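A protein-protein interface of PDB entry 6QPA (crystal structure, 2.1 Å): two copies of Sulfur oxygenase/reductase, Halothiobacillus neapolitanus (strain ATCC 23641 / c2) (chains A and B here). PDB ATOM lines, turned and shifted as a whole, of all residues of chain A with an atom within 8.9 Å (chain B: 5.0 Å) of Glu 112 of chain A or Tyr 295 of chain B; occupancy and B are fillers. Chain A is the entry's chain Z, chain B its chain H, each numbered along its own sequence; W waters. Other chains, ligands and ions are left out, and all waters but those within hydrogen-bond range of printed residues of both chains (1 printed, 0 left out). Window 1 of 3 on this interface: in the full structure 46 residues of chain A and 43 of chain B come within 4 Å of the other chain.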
ATOM      1  N   ASN A  11     -11.239  -3.209  17.065  1.00  0.00           N
ATOM      2  CA  ASN A  11     -12.041  -3.405  15.868  1.00  0.00           C
ATOM      3  C   ASN A  11     -11.884  -4.850  15.421  1.00  0.00           C
ATOM      4  O   ASN A  11     -10.790  -5.257  15.004  1.00  0.00           O
ATOM      5  CB  ASN A  11     -11.604  -2.432  14.777  1.00  0.00           C
ATOM      6  CG  ASN A  11     -12.575  -2.389  13.635  1.00  0.00           C
ATOM      7  OD1 ASN A  11     -12.639  -3.318  12.827  1.00  0.00           O
ATOM      8  ND2 ASN A  11     -13.351  -1.316  13.562  1.00  0.00           N
ATOM      9  N   MET A  12     -12.966  -5.631  15.498  1.00  0.00           N
ATOM     10  CA  MET A  12     -12.907  -7.057  15.203  1.00  0.00           C
ATOM     11  C   MET A  12     -13.565  -7.314  13.862  1.00  0.00           C
ATOM     12  O   MET A  12     -14.718  -6.932  13.648  1.00  0.00           O
ATOM     13  CB  MET A  12     -13.580  -7.873  16.298  1.00  0.00           C
ATOM     14  CG  MET A  12     -12.971  -7.638  17.661  1.00  0.00           C
ATOM     15  SD  MET A  12     -14.067  -8.335  18.919  1.00  0.00           S
ATOM     16  CE  MET A  12     -13.066  -8.135  20.373  1.00  0.00           C
ATOM     17  N   ALA A  13     -12.826  -7.940  12.959  1.00  0.00           N
ATOM     18  CA  ALA A  13     -13.358  -8.291  11.652  1.00  0.00           C
ATOM     19  C   ALA A  13     -12.826  -9.660  11.262  1.00  0.00           C
ATOM     20  O   ALA A  13     -11.863 -10.162  11.844  1.00  0.00           O
ATOM     21  CB  ALA A  13     -12.992  -7.252  10.586  1.00  0.00           C
ATOM     22  N   LYS A  14     -13.510 -10.287  10.313  1.00  0.00           N
ATOM     23  CA  LYS A  14     -13.049 -11.514   9.686  1.00  0.00           C
ATOM     24  C   LYS A  14     -12.927 -11.255   8.195  1.00  0.00           C
ATOM     25  O   LYS A  14     -13.871 -10.765   7.567  1.00  0.00           O
ATOM     26  CB  LYS A  14     -13.993 -12.680   9.981  1.00  0.00           C
ATOM     27  CG  LYS A  14     -13.995 -13.062  11.458  1.00  0.00           C
ATOM     28  CD  LYS A  14     -14.893 -14.251  11.740  1.00  0.00           C
ATOM     29  CE  LYS A  14     -14.755 -14.697  13.187  1.00  0.00           C
ATOM     30  NZ  LYS A  14     -13.340 -15.124  13.449  1.00  0.00           N
ATOM     31  N   ILE A  15     -11.754 -11.534   7.644  1.00  0.00           N
ATOM     32  CA  ILE A  15     -11.465 -11.165   6.275  1.00  0.00           C
ATOM     33  C   ILE A  15     -11.084 -12.393   5.473  1.00  0.00           C
ATOM     34  O   ILE A  15     -10.654 -13.420   6.009  1.00  0.00           O
ATOM     35  CB  ILE A  15     -10.357 -10.096   6.195  1.00  0.00           C
ATOM     36  CG1 ILE A  15      -9.011 -10.665   6.648  1.00  0.00           C
ATOM     37  CG2 ILE A  15     -10.769  -8.871   7.010  1.00  0.00           C
ATOM     38  CD1 ILE A  15      -7.839  -9.644   6.557  1.00  0.00           C
ATOM     39  N   ALA A  16     -11.243 -12.261   4.162  1.00  0.00           N
ATOM     40  CA  ALA A  16     -10.905 -13.340   3.257  1.00  0.00           C
ATOM     41  C   ALA A  16      -9.403 -13.583   3.283  1.00  0.00           C
ATOM     42  O   ALA A  16      -8.609 -12.646   3.244  1.00  0.00           O
ATOM     43  CB  ALA A  16     -11.358 -13.004   1.838  1.00  0.00           C
ATOM     44  N   PRO A  73     -12.901 -17.342   6.756  1.00  0.00           N
ATOM     45  CA  PRO A  73     -12.161 -16.106   6.991  1.00  0.00           C
ATOM     46  C   PRO A  73     -11.129 -16.198   8.110  1.00  0.00           C
ATOM     47  O   PRO A  73     -11.154 -17.125   8.920  1.00  0.00           O
ATOM     48  CB  PRO A  73     -13.262 -15.122   7.391  1.00  0.00           C
ATOM     49  CG  PRO A  73     -14.270 -15.991   8.099  1.00  0.00           C
ATOM     50  CD  PRO A  73     -14.266 -17.285   7.313  1.00  0.00           C
ATOM     51  N   MET A  74     -10.224 -15.226   8.155  1.00  0.00           N
ATOM     52  CA  MET A  74      -9.271 -15.119   9.243  1.00  0.00           C
ATOM     53  C   MET A  74      -9.568 -13.853  10.041  1.00  0.00           C
ATOM     54  O   MET A  74      -9.943 -12.812   9.479  1.00  0.00           O
ATOM     55  CB  MET A  74      -7.829 -15.116   8.725  1.00  0.00           C
ATOM     56  CG  MET A  74      -7.450 -13.905   7.888  1.00  0.00           C
ATOM     57  SD  MET A  74      -5.994 -14.181   6.838  1.00  0.00           S
ATOM     58  CE  MET A  74      -4.999 -15.153   7.958  1.00  0.00           C
ATOM     59  N   GLY A  75      -9.403 -13.949  11.356  1.00  0.00           N
ATOM     60  CA  GLY A  75      -9.630 -12.797  12.207  1.00  0.00           C
ATOM     61  C   GLY A  75      -8.590 -11.709  11.984  1.00  0.00           C
ATOM     62  O   GLY A  75      -7.408 -11.967  11.736  1.00  0.00           O
ATOM     63  N   MET A  76      -9.045 -10.479  12.075  1.00  0.00           N
ATOM     64  CA  MET A  76      -8.175  -9.318  12.013  1.00  0.00           C
ATOM     65  C   MET A  76      -8.634  -8.370  13.109  1.00  0.00           C
ATOM     66  O   MET A  76      -9.756  -7.859  13.051  1.00  0.00           O
ATOM     67  CB  MET A  76      -8.248  -8.672  10.635  1.00  0.00           C
ATOM     68  CG  MET A  76      -6.959  -8.061  10.215  1.00  0.00           C
ATOM     69  SD  MET A  76      -7.155  -6.329  10.499  1.00  0.00           S
ATOM     70  CE  MET A  76      -8.232  -5.927   9.115  1.00  0.00           C
ATOM     71  N   PHE A  77      -7.810  -8.189  14.137  1.00  0.00           N
ATOM     72  CA  PHE A  77      -8.149  -7.329  15.266  1.00  0.00           C
ATOM     73  C   PHE A  77      -7.225  -6.118  15.229  1.00  0.00           C
ATOM     74  O   PHE A  77      -5.999  -6.271  15.188  1.00  0.00           O
ATOM     75  CB  PHE A  77      -7.997  -8.036  16.624  1.00  0.00           C
ATOM     76  CG  PHE A  77      -9.080  -9.061  16.954  1.00  0.00           C
ATOM     77  CD1 PHE A  77      -9.886  -9.621  15.977  1.00  0.00           C
ATOM     78  CD2 PHE A  77      -9.265  -9.468  18.276  1.00  0.00           C
ATOM     79  CE1 PHE A  77     -10.862 -10.564  16.317  1.00  0.00           C
ATOM     80  CE2 PHE A  77     -10.231 -10.418  18.620  1.00  0.00           C
ATOM     81  CZ  PHE A  77     -11.031 -10.966  17.641  1.00  0.00           C
ATOM     82  N   CYS A 106     -12.015  -1.425   2.103  1.00  0.00           N
ATOM     83  CA  CYS A 106     -11.728  -2.659   2.834  1.00  0.00           C
ATOM     84  C   CYS A 106     -12.892  -3.648   2.826  1.00  0.00           C
ATOM     85  O   CYS A 106     -12.661  -4.849   2.996  1.00  0.00           O
ATOM     86  CB  CYS A 106     -11.333  -2.349   4.280  1.00  0.00           C
ATOM     87  SG  CYS A 106      -9.719  -1.547   4.462  1.00  0.00           S
ATOM     88  N   LEU A 107     -14.129  -3.176   2.631  1.00  0.00           N
ATOM     89  CA  LEU A 107     -15.308  -4.036   2.717  1.00  0.00           C
ATOM     90  C   LEU A 107     -15.309  -5.142   1.668  1.00  0.00           C
ATOM     91  O   LEU A 107     -16.027  -6.138   1.836  1.00  0.00           O
ATOM     92  CB  LEU A 107     -16.587  -3.199   2.578  1.00  0.00           C
ATOM     93  CG  LEU A 107     -16.936  -2.357   3.812  1.00  0.00           C
ATOM     94  CD1 LEU A 107     -18.233  -1.585   3.623  1.00  0.00           C
ATOM     95  CD2 LEU A 107     -17.009  -3.211   5.059  1.00  0.00           C
ATOM     96  N   MET A 109     -13.031  -7.193   1.228  1.00  0.00           N
ATOM     97  CA  MET A 109     -12.379  -8.359   1.801  1.00  0.00           C
ATOM     98  C   MET A 109     -13.032  -8.800   3.099  1.00  0.00           C
ATOM     99  O   MET A 109     -12.605  -9.803   3.679  1.00  0.00           O
ATOM    100  CB  MET A 109     -10.888  -8.084   2.048  1.00  0.00           C
ATOM    101  CG  MET A 109     -10.574  -7.199   3.249  1.00  0.00           C
ATOM    102  SD  MET A 109      -8.782  -6.936   3.474  1.00  0.00           S
ATOM    103  CE  MET A 109      -8.743  -5.812   4.870  1.00  0.00           C
ATOM    104  N   VAL A 110     -14.074  -8.102   3.548  1.00  0.00           N
ATOM    105  CA  VAL A 110     -14.692  -8.368   4.838  1.00  0.00           C
ATOM    106  C   VAL A 110     -15.762  -9.439   4.689  1.00  0.00           C
ATOM    107  O   VAL A 110     -16.637  -9.343   3.823  1.00  0.00           O
ATOM    108  CB  VAL A 110     -15.279  -7.083   5.430  1.00  0.00           C
ATOM    109  CG1 VAL A 110     -16.107  -7.407   6.640  1.00  0.00           C
ATOM    110  CG2 VAL A 110     -14.153  -6.121   5.781  1.00  0.00           C
ATOM    111  N   ILE A 111     -15.698 -10.461   5.540  1.00  0.00           N
ATOM    112  CA  ILE A 111     -16.712 -11.498   5.571  1.00  0.00           C
ATOM    113  C   ILE A 111     -17.635 -11.363   6.776  1.00  0.00           C
ATOM    114  O   ILE A 111     -18.817 -11.715   6.680  1.00  0.00           O
ATOM    115  CB  ILE A 111     -16.045 -12.891   5.536  1.00  0.00           C
ATOM    116  CG1 ILE A 111     -15.461 -13.144   4.146  1.00  0.00           C
ATOM    117  CG2 ILE A 111     -17.029 -14.013   5.975  1.00  0.00           C
ATOM    118  CD1 ILE A 111     -14.470 -14.317   4.067  1.00  0.00           C
ATOM    119  N   GLU A 112     -17.134 -10.838   7.892  1.00  0.00           N
ATOM    120  CA  GLU A 112     -17.913 -10.610   9.099  1.00  0.00           C
ATOM    121  C   GLU A 112     -17.312  -9.411   9.814  1.00  0.00           C
ATOM    122  O   GLU A 112     -16.099  -9.177   9.748  1.00  0.00           O
ATOM    123  CB  GLU A 112     -17.915 -11.850  10.003  1.00  0.00           C
ATOM    124  CG  GLU A 112     -18.993 -11.871  11.052  1.00  0.00           C
ATOM    125  CD  GLU A 112     -19.053 -13.206  11.778  1.00  0.00           C
ATOM    126  OE1 GLU A 112     -18.256 -14.116  11.430  1.00  0.00           O
ATOM    127  OE2 GLU A 112     -19.902 -13.331  12.693  1.00  0.00           O
ATOM    128  N   GLY A 113     -18.163  -8.637  10.479  1.00  0.00           N
ATOM    129  CA  GLY A 113     -17.694  -7.437  11.135  1.00  0.00           C
ATOM    130  C   GLY A 113     -17.803  -6.208  10.248  1.00  0.00           C
ATOM    131  O   GLY A 113     -18.442  -6.236   9.192  1.00  0.00           O
ATOM    132  N   PRO A 114     -17.215  -5.082  10.678  1.00  0.00           N
ATOM    133  CA  PRO A 114     -16.491  -4.913  11.933  1.00  0.00           C
ATOM    134  C   PRO A 114     -17.430  -4.745  13.118  1.00  0.00           C
ATOM    135  O   PRO A 114     -18.554  -4.258  12.989  1.00  0.00           O
ATOM    136  CB  PRO A 114     -15.714  -3.618  11.709  1.00  0.00           C
ATOM    137  CG  PRO A 114     -16.678  -2.803  10.884  1.00  0.00           C
ATOM    138  CD  PRO A 114     -17.340  -3.803   9.954  1.00  0.00           C
ATOM    139  N   TRP A 115     -16.937  -5.147  14.274  1.00  0.00           N
ATOM    140  CA  TRP A 115     -17.580  -4.907  15.552  1.00  0.00           C
ATOM    141  C   TRP A 115     -16.496  -4.355  16.460  1.00  0.00           C
ATOM    142  O   TRP A 115     -15.410  -4.939  16.536  1.00  0.00           O
ATOM    143  CB  TRP A 115     -18.174  -6.208  16.088  1.00  0.00           C
ATOM    144  CG  TRP A 115     -18.979  -6.083  17.323  1.00  0.00           C
ATOM    145  CD1 TRP A 115     -18.682  -6.625  18.541  1.00  0.00           C
ATOM    146  CD2 TRP A 115     -20.240  -5.407  17.476  1.00  0.00           C
ATOM    147  NE1 TRP A 115     -19.677  -6.325  19.447  1.00  0.00           N
ATOM    148  CE2 TRP A 115     -20.647  -5.584  18.822  1.00  0.00           C
ATOM    149  CE3 TRP A 115     -21.071  -4.686  16.610  1.00  0.00           C
ATOM    150  CZ2 TRP A 115     -21.836  -5.037  19.333  1.00  0.00           C
ATOM    151  CZ3 TRP A 115     -22.273  -4.133  17.128  1.00  0.00           C
ATOM    152  CH2 TRP A 115     -22.633  -4.326  18.471  1.00  0.00           C
ATOM    153  N   SER A 209     -18.434   0.347  14.663  1.00  0.00           N
ATOM    154  CA  SER A 209     -18.960  -0.931  14.200  1.00  0.00           C
ATOM    155  C   SER A 209     -19.763  -0.803  12.917  1.00  0.00           C
ATOM    156  O   SER A 209     -20.416  -1.769  12.519  1.00  0.00           O
ATOM    157  CB  SER A 209     -19.825  -1.586  15.280  1.00  0.00           C
ATOM    158  OG  SER A 209     -19.075  -1.798  16.457  1.00  0.00           O
ATOM    159  N   GLN A 211     -22.505   0.644  12.453  1.00  0.00           N
ATOM    160  CA  GLN A 211     -23.922   0.472  12.768  1.00  0.00           C
ATOM    161  C   GLN A 211     -24.566   1.855  12.708  1.00  0.00           C
ATOM    162  O   GLN A 211     -24.571   2.603  13.684  1.00  0.00           O
ATOM    163  CB  GLN A 211     -24.097  -0.192  14.132  1.00  0.00           C
ATOM    164  CG  GLN A 211     -23.499  -1.606  14.213  1.00  0.00           C
ATOM    165  CD  GLN A 211     -24.331  -2.667  13.504  1.00  0.00           C
ATOM    166  OE1 GLN A 211     -23.883  -3.807  13.322  1.00  0.00           O
ATOM    167  NE2 GLN A 211     -25.560  -2.307  13.119  1.00  0.00           N
ATOM    168  N   ILE B  53     -22.945 -16.647   2.742  1.00  0.00           N
ATOM    169  CA  ILE B  53     -23.559 -15.491   3.401  1.00  0.00           C
ATOM    170  C   ILE B  53     -24.235 -14.617   2.348  1.00  0.00           C
ATOM    171  O   ILE B  53     -24.064 -14.811   1.142  1.00  0.00           O
ATOM    172  CB  ILE B  53     -22.559 -14.619   4.189  1.00  0.00           C
ATOM    173  CG1 ILE B  53     -21.631 -13.876   3.222  1.00  0.00           C
ATOM    174  CG2 ILE B  53     -21.734 -15.444   5.162  1.00  0.00           C
ATOM    175  CD1 ILE B  53     -20.880 -12.732   3.879  1.00  0.00           C
ATOM    176  N   TYR B  60     -20.556  -6.984   3.043  1.00  0.00           N
ATOM    177  CA  TYR B  60     -19.638  -8.070   3.376  1.00  0.00           C
ATOM    178  C   TYR B  60     -19.064  -8.612   2.074  1.00  0.00           C
ATOM    179  O   TYR B  60     -19.316  -9.765   1.706  1.00  0.00           O
ATOM    180  CB  TYR B  60     -20.345  -9.168   4.187  1.00  0.00           C
ATOM    181  CG  TYR B  60     -21.066  -8.618   5.399  1.00  0.00           C
ATOM    182  CD1 TYR B  60     -20.362  -8.224   6.530  1.00  0.00           C
ATOM    183  CD2 TYR B  60     -22.448  -8.451   5.398  1.00  0.00           C
ATOM    184  CE1 TYR B  60     -21.013  -7.690   7.635  1.00  0.00           C
ATOM    185  CE2 TYR B  60     -23.105  -7.924   6.501  1.00  0.00           C
ATOM    186  CZ  TYR B  60     -22.373  -7.535   7.615  1.00  0.00           C
ATOM    187  OH  TYR B  60     -23.011  -7.010   8.721  1.00  0.00           O
ATOM    188  N   ILE B 162     -30.321 -17.568   7.912  1.00  0.00           N
ATOM    189  CA  ILE B 162     -30.478 -17.115   9.291  1.00  0.00           C
ATOM    190  C   ILE B 162     -29.874 -15.727   9.431  1.00  0.00           C
ATOM    191  O   ILE B 162     -28.670 -15.537   9.228  1.00  0.00           O
ATOM    192  CB  ILE B 162     -29.837 -18.078  10.296  1.00  0.00           C
ATOM    193  CG1 ILE B 162     -30.465 -19.464  10.173  1.00  0.00           C
ATOM    194  CG2 ILE B 162     -30.018 -17.516  11.696  1.00  0.00           C
ATOM    195  CD1 ILE B 162     -29.840 -20.479  11.078  1.00  0.00           C
ATOM    196  N   GLY B 163     -30.723 -14.752   9.789  1.00  0.00           N
ATOM    197  CA  GLY B 163     -30.293 -13.392  10.006  1.00  0.00           C
ATOM    198  C   GLY B 163     -30.127 -13.100  11.481  1.00  0.00           C
ATOM    199  O   GLY B 163     -31.081 -13.196  12.255  1.00  0.00           O
ATOM    200  N   ASP B 164     -28.907 -12.745  11.860  1.00  0.00           N
ATOM    201  CA  ASP B 164     -28.538 -12.475  13.246  1.00  0.00           C
ATOM    202  C   ASP B 164     -28.793 -11.006  13.550  1.00  0.00           C
ATOM    203  O   ASP B 164     -28.311 -10.134  12.825  1.00  0.00           O
ATOM    204  CB  ASP B 164     -27.070 -12.858  13.454  1.00  0.00           C
ATOM    205  CG  ASP B 164     -26.672 -12.941  14.921  1.00  0.00           C
ATOM    206  OD1 ASP B 164     -27.383 -12.367  15.785  1.00  0.00           O
ATOM    207  OD2 ASP B 164     -25.634 -13.570  15.206  1.00  0.00           O
ATOM    208  N   GLY B 293     -26.154  -6.030  13.427  1.00  0.00           N
ATOM    209  CA  GLY B 293     -26.797  -6.713  12.327  1.00  0.00           C
ATOM    210  C   GLY B 293     -27.528  -5.779  11.370  1.00  0.00           C
ATOM    211  O   GLY B 293     -27.413  -4.552  11.440  1.00  0.00           O
ATOM    212  N   PRO B 294     -28.314  -6.352  10.451  1.00  0.00           N
ATOM    213  CA  PRO B 294     -28.495  -7.791  10.311  1.00  0.00           C
ATOM    214  C   PRO B 294     -27.316  -8.466   9.597  1.00  0.00           C
ATOM    215  O   PRO B 294     -26.623  -7.833   8.813  1.00  0.00           O
ATOM    216  CB  PRO B 294     -29.783  -7.904   9.496  1.00  0.00           C
ATOM    217  CG  PRO B 294     -29.899  -6.645   8.754  1.00  0.00           C
ATOM    218  CD  PRO B 294     -29.198  -5.582   9.557  1.00  0.00           C
ATOM    219  N   TYR B 295     -27.069  -9.736   9.921  1.00  0.00           N
ATOM    220  CA  TYR B 295     -26.056 -10.544   9.250  1.00  0.00           C
ATOM    221  C   TYR B 295     -26.698 -11.869   8.875  1.00  0.00           C
ATOM    222  O   TYR B 295     -27.182 -12.593   9.754  1.00  0.00           O
ATOM    223  CB  TYR B 295     -24.843 -10.770  10.151  1.00  0.00           C
ATOM    224  CG  TYR B 295     -23.707 -11.501   9.481  1.00  0.00           C
ATOM    225  CD1 TYR B 295     -22.874 -10.839   8.578  1.00  0.00           C
ATOM    226  CD2 TYR B 295     -23.459 -12.853   9.745  1.00  0.00           C
ATOM    227  CE1 TYR B 295     -21.819 -11.507   7.944  1.00  0.00           C
ATOM    228  CE2 TYR B 295     -22.400 -13.527   9.117  1.00  0.00           C
ATOM    229  CZ  TYR B 295     -21.593 -12.846   8.220  1.00  0.00           C
ATOM    230  OH  TYR B 295     -20.544 -13.493   7.609  1.00  0.00           O
ATOM    231  N   TYR B 296     -26.682 -12.203   7.587  1.00  0.00           N
ATOM    232  CA  TYR B 296     -27.394 -13.367   7.073  1.00  0.00           C
ATOM    233  C   TYR B 296     -26.414 -14.454   6.641  1.00  0.00           C
ATOM    234  O   TYR B 296     -25.646 -14.262   5.695  1.00  0.00           O
ATOM    235  CB  TYR B 296     -28.304 -12.956   5.919  1.00  0.00           C
ATOM    236  CG  TYR B 296     -29.619 -12.402   6.414  1.00  0.00           C
ATOM    237  CD1 TYR B 296     -30.654 -13.257   6.741  1.00  0.00           C
ATOM    238  CD2 TYR B 296     -29.805 -11.051   6.606  1.00  0.00           C
ATOM    239  CE1 TYR B 296     -31.866 -12.792   7.212  1.00  0.00           C
ATOM    240  CE2 TYR B 296     -31.013 -10.560   7.087  1.00  0.00           C
ATOM    241  CZ  TYR B 296     -32.042 -11.441   7.391  1.00  0.00           C
ATOM    242  OH  TYR B 296     -33.261 -10.999   7.870  1.00  0.00           O
ATOM    243  N   MET B 297     -26.475 -15.604   7.308  1.00  0.00           N
ATOM    244  CA  MET B 297     -25.723 -16.776   6.894  1.00  0.00           C
ATOM    245  C   MET B 297     -26.642 -17.683   6.090  1.00  0.00           C
ATOM    246  O   MET B 297     -27.817 -17.830   6.429  1.00  0.00           O
ATOM    247  CB  MET B 297     -25.179 -17.529   8.105  1.00  0.00           C
ATOM    248  CG  MET B 297     -24.276 -16.687   8.998  1.00  0.00           C
ATOM    249  SD  MET B 297     -23.910 -17.457  10.591  1.00  0.00           S
ATOM    250  CE  MET B 297     -22.955 -18.869  10.044  1.00  0.00           C
HETATM  251  O   HOH W   1     -24.023  -5.622  10.871  1.00  0.00           O
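The side-chain hydroxyl of Tyr 295 of chain B sits at hydrogen-bond distance from the backbone carbonyl oxygen of Ile 111 of chain A. The backbone NH (N) of Gly 293 of chain B sits at hydrogen-bond distance from the side-chain amide oxygen (OE1) of Gln 211 of chain A, 3.2 Å away. The backbone carbonyl oxygen (O) of Val 110 of chain A lies close to the backbone carbonyl oxygen (O) of Tyr 60 of chain B.
The backbone carbonyl oxygen of Lys 14 of chain A is in hydrogen-bond range of the backbone NH of Ile 111 of chain A (2.7 Å). The backbone NH (N) of Lys 14 of chain A is in hydrogen-bond range of the backbone carbonyl oxygen (O) of Glu 112 of chain A (2.9 Å). O of Tyr 295 of chain B is in hydrogen-bond range of N of Asp 164 of chain B.
Among the printed residues, merely in contact across the chains: Gly 113 of chain A with Tyr 60 of chain B (3.3 Å), Ile 111 of chain A with Ile 53 of chain B (3.6 Å), Ile 111 of chain A with Tyr 60 of chain B (3.8 Å), Glu 112 of chain A with Tyr 295 of chain B (3.9 Å) and Leu 107 of chain A with Tyr 60 of chain B (3.9 Å).
Of the printed residues of chain B, Ile 111 of chain A touches Ile 53 (3.6 Å), Tyr 60 (3.8 Å) and Tyr 295 (2.6 Å). Glu 112 of chain A touches one residue of chain B. Of the printed residues of chain B, Gly 113 of chain A touches Tyr 60. Printed residues of chain A within 4 Å of Tyr 60 of chain B: Leu 107, Val 110, Ile 111 and Gly 113. No residue of chain A comes within 4 Å of Gly 163 of chain B. No residue of chain A comes within 4 Å of Pro 294 of chain B. Of the printed residues of chain A, Tyr 295 of chain B touches Ile 111 and Glu 112. The nearest residue of chain B that does not touch Glu 112 of chain A is Tyr 60 of chain B (4.3 Å). The nearest residue of chain A that does not touch Tyr 295 of chain B is Gly 113 of chain A (5.3 Å). The nearest printed residue of chain A that does not touch Ile 53 of chain B is Val 110 of chain A (5.4 Å).
Of the 22 printed residues of chain A, 6 touch a printed residue of chain B. Hydrophobic or aromatic side chains of chain A within 4 Å of the printed part of chain B: Ile 111. Printed residues of chain B that touch a printed residue of chain A: Ile 53, Tyr 60, Gly 293 and Tyr 295. Hydrophobic or aromatic side chains of chain B that line the printed part of chain A: Ile 53, Tyr 60 and Tyr 295. Among the printed residues, 8 pairs touch across the chains. Among the printed residues, no Asp or Glu carboxylate lies within 4 Å of a Lys or Arg side-chain nitrogen of the other chain.
No position is printed for both chains.
Water W1 lies within hydrogen-bond range of the side-chain hydroxyl (OH) of Tyr 60 of chain B (2.8 Å), the side-chain amide oxygen (OE1) of Gln 211 of chain A (3.1 Å) and the backbone NH (N) of Gly 293 of chain B (3.4 Å).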
